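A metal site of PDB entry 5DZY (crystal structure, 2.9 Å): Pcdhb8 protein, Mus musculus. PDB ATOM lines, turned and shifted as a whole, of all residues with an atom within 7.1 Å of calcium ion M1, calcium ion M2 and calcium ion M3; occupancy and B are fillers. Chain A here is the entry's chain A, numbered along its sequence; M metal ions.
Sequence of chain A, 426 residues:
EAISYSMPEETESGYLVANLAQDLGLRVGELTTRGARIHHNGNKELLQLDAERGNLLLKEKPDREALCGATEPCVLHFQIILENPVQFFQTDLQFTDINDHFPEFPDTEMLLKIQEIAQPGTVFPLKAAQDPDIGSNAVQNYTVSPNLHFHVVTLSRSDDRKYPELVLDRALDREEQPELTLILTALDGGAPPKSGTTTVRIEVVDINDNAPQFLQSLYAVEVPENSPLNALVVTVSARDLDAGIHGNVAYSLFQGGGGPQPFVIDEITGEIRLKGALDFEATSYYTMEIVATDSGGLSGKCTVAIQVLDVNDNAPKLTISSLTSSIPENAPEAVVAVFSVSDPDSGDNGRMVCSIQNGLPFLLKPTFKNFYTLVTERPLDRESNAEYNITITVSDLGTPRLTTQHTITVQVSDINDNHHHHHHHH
The nearest printed residue that does not touch calcium ion M2 is Arg 64 (4.7 Å).
Calcium ion M1 is bound by OD2 of Asp 131, OD2 of Asp 188, OD2 of Asp 133, O of His 101, OD1 of Asn 99 and O of Asn 137. Calcium ion M1 has six donor atoms within binding distance. Slightly farther from calcium ion M1 lies the side-chain carboxylate (OD1) of Asp 131 (2.9 Å).
OD2 of Asp 63 is in hydrogen-bond range of N of Ala 66 (3.1 Å). The side-chain carboxylate of Glu 65 lies close to a ring nitrogen (NE2) of His 101 (3.4 Å). The backbone NH (N) of Gly 190 sits at hydrogen-bond distance from the side-chain carboxylate (OD1) of Asp 188, at 3.0 Å. The side-chain carboxylate (OD2) of Asp 97 sits at hydrogen-bond distance from the side-chain amide nitrogen (ND2) of Asn 137 (2.8 Å). The side-chain carboxylate (OD1) of Asp 97 sits close to the guanidinium group (NH1) of Arg 64. The side-chain carboxylate (OD1) of Asp 63 lies close to the side-chain carboxylate (OE2) of Glu 10, at 2.6 Å. The backbone carbonyl oxygen (O) of Lys 194 is in hydrogen-bond range of the backbone NH (N) of Asp 188, 2.8 Å away. The side-chain carboxylate of Glu 9 is in hydrogen-bond range of the backbone NH of Arg 64 (2.9 Å).
Merely in contact with calcium ion M3: Glu 10. Within 4 Å of calcium ion M3: Glu 9, Glu 10, Asp 63, Glu 65, Asp 100 and His 101. The nearest printed residue that does not touch calcium ion M3 is Arg 64 (5.2 Å).
Calcium ion M3 is bound by the side-chain carboxylate (OD2) of Asp 100 (2.2 Å), the side-chain carboxylate (OD1) of Asp 63 (2.5 Å) and the side-chain carboxylate (OE1) of Glu 65 (2.7 Å). Slightly farther from calcium ion M3 lies OE2 of Glu 9 (2.9 Å). Slightly farther from calcium ion M3 lies NE2 of His 101 (3.0 Å). Slightly farther from calcium ion M3 lies OD1 of Asp 100 (3.1 Å).
Within 4 Å of calcium ion M1: Asn 99, His 101, Asp 131, Asp 133, Asn 137 and Asp 188.
Calcium ion M2 is bound by the side-chain carboxylate (OE2) of Glu 65. OD1 of Asp 100 binds calcium ion M2, at 2.5 Å. The side-chain carboxylate (OD1) of Asp 97 binds calcium ion M2. O of Ile 98 is bound to calcium ion M2 (2.6 Å). The side-chain carboxylate (OD1) of Asp 133 is bound to calcium ion M2 (2.8 Å). OE1 of Glu 9 is bound to calcium ion M2, 2.8 Å away.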
ATOM      1  N   GLU A   9      14.957  -5.726  18.240  1.00  0.00           N
ATOM      2  CA  GLU A   9      15.555  -6.332  19.422  1.00  0.00           C
ATOM      3  C   GLU A   9      14.654  -6.162  20.645  1.00  0.00           C
ATOM      4  O   GLU A   9      13.808  -5.276  20.688  1.00  0.00           O
ATOM      5  CB  GLU A   9      16.929  -5.703  19.691  1.00  0.00           C
ATOM      6  CG  GLU A   9      17.741  -6.372  20.793  1.00  0.00           C
ATOM      7  CD  GLU A   9      18.921  -5.526  21.240  1.00  0.00           C
ATOM      8  OE1 GLU A   9      19.190  -4.486  20.586  1.00  0.00           O
ATOM      9  OE2 GLU A   9      19.577  -5.895  22.229  1.00  0.00           O
ATOM     10  N   GLU A  10      14.837  -7.038  21.638  1.00  0.00           N
ATOM     11  CA  GLU A  10      14.146  -6.950  22.921  1.00  0.00           C
ATOM     12  C   GLU A  10      12.632  -6.989  22.793  1.00  0.00           C
ATOM     13  O   GLU A  10      11.917  -6.336  23.552  1.00  0.00           O
ATOM     14  CB  GLU A  10      14.568  -5.672  23.661  1.00  0.00           C
ATOM     15  CG  GLU A  10      16.027  -5.647  24.104  1.00  0.00           C
ATOM     16  CD  GLU A  10      16.284  -6.487  25.337  1.00  0.00           C
ATOM     17  OE1 GLU A  10      15.317  -7.039  25.902  1.00  0.00           O
ATOM     18  OE2 GLU A  10      17.459  -6.589  25.749  1.00  0.00           O
ATOM     19  N   PRO A  62      15.031 -11.945  23.187  1.00  0.00           N
ATOM     20  CA  PRO A  62      16.391 -11.847  22.641  1.00  0.00           C
ATOM     21  C   PRO A  62      17.082 -10.512  22.913  1.00  0.00           C
ATOM     22  O   PRO A  62      16.431  -9.465  22.923  1.00  0.00           O
ATOM     23  CB  PRO A  62      16.157 -12.034  21.135  1.00  0.00           C
ATOM     24  CG  PRO A  62      14.817 -11.431  20.913  1.00  0.00           C
ATOM     25  CD  PRO A  62      14.008 -11.716  22.151  1.00  0.00           C
ATOM     26  N   ASP A  63      18.392 -10.568  23.139  1.00  0.00           N
ATOM     27  CA  ASP A  63      19.204  -9.363  23.289  1.00  0.00           C
ATOM     28  C   ASP A  63      20.389  -9.429  22.339  1.00  0.00           C
ATOM     29  O   ASP A  63      21.248 -10.301  22.463  1.00  0.00           O
ATOM     30  CB  ASP A  63      19.685  -9.220  24.732  1.00  0.00           C
ATOM     31  CG  ASP A  63      20.552  -7.984  24.935  1.00  0.00           C
ATOM     32  OD1 ASP A  63      19.997  -6.894  25.180  1.00  0.00           O
ATOM     33  OD2 ASP A  63      21.794  -8.119  24.846  1.00  0.00           O
ATOM     34  N   ARG A  64      20.428  -8.499  21.390  1.00  0.00           N
ATOM     35  CA  ARG A  64      21.415  -8.504  20.310  1.00  0.00           C
ATOM     36  C   ARG A  64      22.853  -8.522  20.827  1.00  0.00           C
ATOM     37  O   ARG A  64      23.673  -9.313  20.359  1.00  0.00           O
ATOM     38  CB  ARG A  64      21.199  -7.288  19.403  1.00  0.00           C
ATOM     39  CG  ARG A  64      21.562  -7.503  17.928  1.00  0.00           C
ATOM     40  CD  ARG A  64      23.065  -7.547  17.710  1.00  0.00           C
ATOM     41  NE  ARG A  64      23.753  -6.511  18.475  1.00  0.00           N
ATOM     42  CZ  ARG A  64      23.916  -5.260  18.066  1.00  0.00           C
ATOM     43  NH1 ARG A  64      24.567  -4.388  18.830  1.00  0.00           N
ATOM     44  NH2 ARG A  64      23.437  -4.874  16.895  1.00  0.00           N
ATOM     45  N   GLU A  65      23.140  -7.654  21.781  1.00  0.00           N
ATOM     46  CA  GLU A  65      24.501  -7.508  22.299  1.00  0.00           C
ATOM     47  C   GLU A  65      25.010  -8.779  22.967  1.00  0.00           C
ATOM     48  O   GLU A  65      26.216  -9.021  23.035  1.00  0.00           O
ATOM     49  CB  GLU A  65      24.578  -6.339  23.284  1.00  0.00           C
ATOM     50  CG  GLU A  65      24.446  -4.962  22.641  1.00  0.00           C
ATOM     51  CD  GLU A  65      23.034  -4.646  22.196  1.00  0.00           C
ATOM     52  OE1 GLU A  65      22.086  -5.041  22.911  1.00  0.00           O
ATOM     53  OE2 GLU A  65      22.861  -4.019  21.132  1.00  0.00           O
ATOM     54  N   ALA A  66      24.090  -9.601  23.455  1.00  0.00           N
ATOM     55  CA  ALA A  66      24.443 -10.858  24.107  1.00  0.00           C
ATOM     56  C   ALA A  66      24.440 -12.012  23.116  1.00  0.00           C
ATOM     57  O   ALA A  66      24.975 -13.092  23.398  1.00  0.00           O
ATOM     58  CB  ALA A  66      23.499 -11.143  25.261  1.00  0.00           C
ATOM     59  N   THR A  96      16.976  -6.623  14.325  1.00  0.00           N
ATOM     60  CA  THR A  96      17.305  -5.216  14.174  1.00  0.00           C
ATOM     61  C   THR A  96      17.647  -4.598  15.533  1.00  0.00           C
ATOM     62  O   THR A  96      16.858  -4.678  16.468  1.00  0.00           O
ATOM     63  CB  THR A  96      16.155  -4.420  13.533  1.00  0.00           C
ATOM     64  OG1 THR A  96      15.938  -4.898  12.198  1.00  0.00           O
ATOM     65  CG2 THR A  96      16.481  -2.937  13.479  1.00  0.00           C
ATOM     66  N   ASP A  97      18.832  -3.988  15.613  1.00  0.00           N
ATOM     67  CA  ASP A  97      19.293  -3.402  16.869  1.00  0.00           C
ATOM     68  C   ASP A  97      18.455  -2.184  17.259  1.00  0.00           C
ATOM     69  O   ASP A  97      18.065  -1.387  16.416  1.00  0.00           O
ATOM     70  CB  ASP A  97      20.768  -3.000  16.747  1.00  0.00           C
ATOM     71  CG  ASP A  97      21.281  -2.321  17.999  1.00  0.00           C
ATOM     72  OD1 ASP A  97      21.815  -3.029  18.886  1.00  0.00           O
ATOM     73  OD2 ASP A  97      21.162  -1.081  18.100  1.00  0.00           O
ATOM     74  N   ILE A  98      18.199  -2.060  18.560  1.00  0.00           N
ATOM     75  CA  ILE A  98      17.487  -0.904  19.089  1.00  0.00           C
ATOM     76  C   ILE A  98      18.385  -0.111  20.033  1.00  0.00           C
ATOM     77  O   ILE A  98      19.393  -0.625  20.521  1.00  0.00           O
ATOM     78  CB  ILE A  98      16.201  -1.319  19.845  1.00  0.00           C
ATOM     79  CG1 ILE A  98      16.558  -2.144  21.077  1.00  0.00           C
ATOM     80  CG2 ILE A  98      15.272  -2.086  18.919  1.00  0.00           C
ATOM     81  CD1 ILE A  98      15.363  -2.504  21.935  1.00  0.00           C
ATOM     82  N   ASN A  99      18.026   1.144  20.276  1.00  0.00           N
ATOM     83  CA  ASN A  99      18.797   1.991  21.171  1.00  0.00           C
ATOM     84  C   ASN A  99      18.381   1.773  22.628  1.00  0.00           C
ATOM     85  O   ASN A  99      17.712   2.626  23.219  1.00  0.00           O
ATOM     86  CB  ASN A  99      18.642   3.465  20.787  1.00  0.00           C
ATOM     87  CG  ASN A  99      19.589   4.375  21.546  1.00  0.00           C
ATOM     88  OD1 ASN A  99      20.596   3.921  22.080  1.00  0.00           O
ATOM     89  ND2 ASN A  99      19.264   5.661  21.594  1.00  0.00           N
ATOM     90  N   ASP A 100      18.767   0.640  23.185  1.00  0.00           N
ATOM     91  CA  ASP A 100      18.394   0.288  24.555  1.00  0.00           C
ATOM     92  C   ASP A 100      19.594   0.310  25.493  1.00  0.00           C
ATOM     93  O   ASP A 100      19.565  -0.304  26.564  1.00  0.00           O
ATOM     94  CB  ASP A 100      17.715  -1.080  24.578  1.00  0.00           C
ATOM     95  CG  ASP A 100      18.586  -2.172  23.970  1.00  0.00           C
ATOM     96  OD1 ASP A 100      19.513  -1.843  23.205  1.00  0.00           O
ATOM     97  OD2 ASP A 100      18.329  -3.356  24.257  1.00  0.00           O
ATOM     98  N   HIS A 101      20.649   1.005  25.088  1.00  0.00           N
ATOM     99  CA  HIS A 101      21.848   1.143  25.914  1.00  0.00           C
ATOM    100  C   HIS A 101      22.218   2.605  26.100  1.00  0.00           C
ATOM    101  O   HIS A 101      22.348   3.353  25.120  1.00  0.00           O
ATOM    102  CB  HIS A 101      23.016   0.373  25.306  1.00  0.00           C
ATOM    103  CG  HIS A 101      23.017  -1.090  25.623  1.00  0.00           C
ATOM    104  ND1 HIS A 101      23.708  -1.628  26.685  1.00  0.00           N
ATOM    105  CD2 HIS A 101      22.395  -2.131  25.012  1.00  0.00           C
ATOM    106  CE1 HIS A 101      23.517  -2.938  26.717  1.00  0.00           C
ATOM    107  NE2 HIS A 101      22.727  -3.264  25.712  1.00  0.00           N
ATOM    108  N   PHE A 102      22.384   3.027  27.350  1.00  0.00           N
ATOM    109  CA  PHE A 102      22.813   4.387  27.650  1.00  0.00           C
ATOM    110  C   PHE A 102      24.334   4.500  27.581  1.00  0.00           C
ATOM    111  O   PHE A 102      25.038   3.617  28.054  1.00  0.00           O
ATOM    112  CB  PHE A 102      22.310   4.822  29.028  1.00  0.00           C
ATOM    113  CG  PHE A 102      20.840   5.108  29.080  1.00  0.00           C
ATOM    114  CD1 PHE A 102      20.105   5.272  27.915  1.00  0.00           C
ATOM    115  CD2 PHE A 102      20.189   5.230  30.301  1.00  0.00           C
ATOM    116  CE1 PHE A 102      18.749   5.545  27.966  1.00  0.00           C
ATOM    117  CE2 PHE A 102      18.833   5.503  30.352  1.00  0.00           C
ATOM    118  CZ  PHE A 102      18.121   5.660  29.181  1.00  0.00           C
ATOM    119  N   PRO A 103      24.829   5.599  26.993  1.00  0.00           N
ATOM    120  CA  PRO A 103      26.269   5.873  26.945  1.00  0.00           C
ATOM    121  C   PRO A 103      26.870   5.935  28.351  1.00  0.00           C
ATOM    122  O   PRO A 103      26.386   6.696  29.191  1.00  0.00           O
ATOM    123  CB  PRO A 103      26.346   7.241  26.256  1.00  0.00           C
ATOM    124  CG  PRO A 103      25.095   7.321  25.452  1.00  0.00           C
ATOM    125  CD  PRO A 103      24.048   6.611  26.263  1.00  0.00           C
ATOM    126  N   GLN A 130      31.456   4.749  25.912  1.00  0.00           N
ATOM    127  CA  GLN A 130      31.234   3.500  25.179  1.00  0.00           C
ATOM    128  C   GLN A 130      29.750   3.169  25.062  1.00  0.00           C
ATOM    129  O   GLN A 130      28.958   3.462  25.958  1.00  0.00           O
ATOM    130  CB  GLN A 130      31.985   2.357  25.861  1.00  0.00           C
ATOM    131  CG  GLN A 130      33.497   2.522  25.847  1.00  0.00           C
ATOM    132  CD  GLN A 130      34.217   1.392  26.545  1.00  0.00           C
ATOM    133  OE1 GLN A 130      33.618   0.626  27.298  1.00  0.00           O
ATOM    134  NE2 GLN A 130      35.522   1.292  26.307  1.00  0.00           N
ATOM    135  N   ASP A 131      29.387   2.550  23.943  1.00  0.00           N
ATOM    136  CA  ASP A 131      28.000   2.176  23.685  1.00  0.00           C
ATOM    137  C   ASP A 131      27.948   0.891  22.878  1.00  0.00           C
ATOM    138  O   ASP A 131      28.367   0.855  21.715  1.00  0.00           O
ATOM    139  CB  ASP A 131      27.281   3.304  22.937  1.00  0.00           C
ATOM    140  CG  ASP A 131      25.771   3.252  23.114  1.00  0.00           C
ATOM    141  OD1 ASP A 131      25.228   2.141  23.276  1.00  0.00           O
ATOM    142  OD2 ASP A 131      25.133   4.323  23.088  1.00  0.00           O
ATOM    143  N   PRO A 132      27.427  -0.188  23.494  1.00  0.00           N
ATOM    144  CA  PRO A 132      27.360  -1.527  22.893  1.00  0.00           C
ATOM    145  C   PRO A 132      26.487  -1.604  21.641  1.00  0.00           C
ATOM    146  O   PRO A 132      26.471  -2.645  20.974  1.00  0.00           O
ATOM    147  CB  PRO A 132      26.760  -2.389  24.014  1.00  0.00           C
ATOM    148  CG  PRO A 132      27.044  -1.626  25.264  1.00  0.00           C
ATOM    149  CD  PRO A 132      26.946  -0.194  24.887  1.00  0.00           C
ATOM    150  N   ASP A 133      25.764  -0.529  21.325  1.00  0.00           N
ATOM    151  CA  ASP A 133      24.882  -0.509  20.173  1.00  0.00           C
ATOM    152  C   ASP A 133      25.652  -0.437  18.857  1.00  0.00           C
ATOM    153  O   ASP A 133      26.888  -0.445  18.850  1.00  0.00           O
ATOM    154  CB  ASP A 133      23.917   0.671  20.262  1.00  0.00           C
ATOM    155  CG  ASP A 133      23.090   0.652  21.542  1.00  0.00           C
ATOM    156  OD1 ASP A 133      22.849  -0.454  22.072  1.00  0.00           O
ATOM    157  OD2 ASP A 133      22.696   1.737  22.008  1.00  0.00           O
ATOM    158  N   ILE A 134      24.928  -0.370  17.747  1.00  0.00           N
ATOM    159  CA  ILE A 134      25.542  -0.355  16.419  1.00  0.00           C
ATOM    160  C   ILE A 134      24.935   0.715  15.522  1.00  0.00           C
ATOM    161  O   ILE A 134      23.714   0.826  15.408  1.00  0.00           O
ATOM    162  CB  ILE A 134      25.412  -1.735  15.721  1.00  0.00           C
ATOM    163  CG1 ILE A 134      26.298  -2.773  16.426  1.00  0.00           C
ATOM    164  CG2 ILE A 134      25.778  -1.638  14.255  1.00  0.00           C
ATOM    165  CD1 ILE A 134      26.392  -4.090  15.682  1.00  0.00           C
ATOM    166  N   SER A 136      23.666   4.202  14.164  1.00  0.00           N
ATOM    167  CA  SER A 136      23.078   5.438  14.682  1.00  0.00           C
ATOM    168  C   SER A 136      22.697   5.298  16.152  1.00  0.00           C
ATOM    169  O   SER A 136      22.527   6.299  16.854  1.00  0.00           O
ATOM    170  CB  SER A 136      21.857   5.825  13.849  1.00  0.00           C
ATOM    171  OG  SER A 136      21.290   7.036  14.328  1.00  0.00           O
ATOM    172  N   ASN A 137      22.582   4.057  16.611  1.00  0.00           N
ATOM    173  CA  ASN A 137      22.235   3.789  18.004  1.00  0.00           C
ATOM    174  C   ASN A 137      23.454   3.898  18.921  1.00  0.00           C
ATOM    175  O   ASN A 137      23.325   3.816  20.145  1.00  0.00           O
ATOM    176  CB  ASN A 137      21.602   2.404  18.134  1.00  0.00           C
ATOM    177  CG  ASN A 137      20.287   2.300  17.394  1.00  0.00           C
ATOM    178  OD1 ASN A 137      19.533   3.278  17.288  1.00  0.00           O
ATOM    179  ND2 ASN A 137      19.990   1.108  16.888  1.00  0.00           N
ATOM    180  N   ALA A 138      24.629   4.077  18.329  1.00  0.00           N
ATOM    181  CA  ALA A 138      25.861   4.214  19.089  1.00  0.00           C
ATOM    182  C   ALA A 138      26.171   5.681  19.377  1.00  0.00           C
ATOM    183  O   ALA A 138      25.337   6.556  19.146  1.00  0.00           O
ATOM    184  CB  ALA A 138      27.018   3.562  18.347  1.00  0.00           C
ATOM    185  N   VAL A 139      27.361   5.939  19.895  1.00  0.00           N
ATOM    186  CA  VAL A 139      27.780   7.305  20.204  1.00  0.00           C
ATOM    187  C   VAL A 139      27.874   8.150  18.941  1.00  0.00           C
ATOM    188  O   VAL A 139      28.434   7.731  17.932  1.00  0.00           O
ATOM    189  CB  VAL A 139      29.139   7.325  20.935  1.00  0.00           C
ATOM    190  CG1 VAL A 139      28.957   6.988  22.401  1.00  0.00           C
ATOM    191  CG2 VAL A 139      30.120   6.367  20.277  1.00  0.00           C
ATOM    192  N   ASP A 188      23.585  10.311  21.999  1.00  0.00           N
ATOM    193  CA  ASP A 188      23.355   9.246  21.037  1.00  0.00           C
ATOM    194  C   ASP A 188      22.720   9.810  19.773  1.00  0.00           C
ATOM    195  O   ASP A 188      22.185  10.914  19.778  1.00  0.00           O
ATOM    196  CB  ASP A 188      22.466   8.156  21.659  1.00  0.00           C
ATOM    197  CG  ASP A 188      22.519   6.839  20.908  1.00  0.00           C
ATOM    198  OD1 ASP A 188      22.588   6.859  19.657  1.00  0.00           O
ATOM    199  OD2 ASP A 188      22.494   5.787  21.563  1.00  0.00           O
ATOM    200  N   GLY A 189      22.774   9.041  18.684  1.00  0.00           N
ATOM    201  CA  GLY A 189      22.203   9.470  17.419  1.00  0.00           C
ATOM    202  C   GLY A 189      20.834   8.875  17.165  1.00  0.00           C
ATOM    203  O   GLY A 189      20.240   9.074  16.100  1.00  0.00           O
ATOM    204  N   GLY A 190      20.325   8.119  18.139  1.00  0.00           N
ATOM    205  CA  GLY A 190      19.033   7.484  18.017  1.00  0.00           C
ATOM    206  C   GLY A 190      17.892   8.438  18.320  1.00  0.00           C
ATOM    207  O   GLY A 190      18.104   9.602  18.656  1.00  0.00           O
ATOM    208  N   LYS A 194      20.017   9.166  23.571  1.00  0.00           N
ATOM    209  CA  LYS A 194      20.378   8.791  24.927  1.00  0.00           C
ATOM    210  C   LYS A 194      21.654   9.506  25.348  1.00  0.00           C
ATOM    211  O   LYS A 194      22.546   9.739  24.537  1.00  0.00           O
ATOM    212  CB  LYS A 194      20.567   7.271  25.027  1.00  0.00           C
HETATM  213 CA    CA M   1      22.970   3.898  22.791  1.00  0.00          CA
HETATM  214 CA    CA M   2      21.045  -2.451  21.269  1.00  0.00          CA
HETATM  215 CA    CA M   3      20.212  -4.473  24.712  1.00  0.00          CA
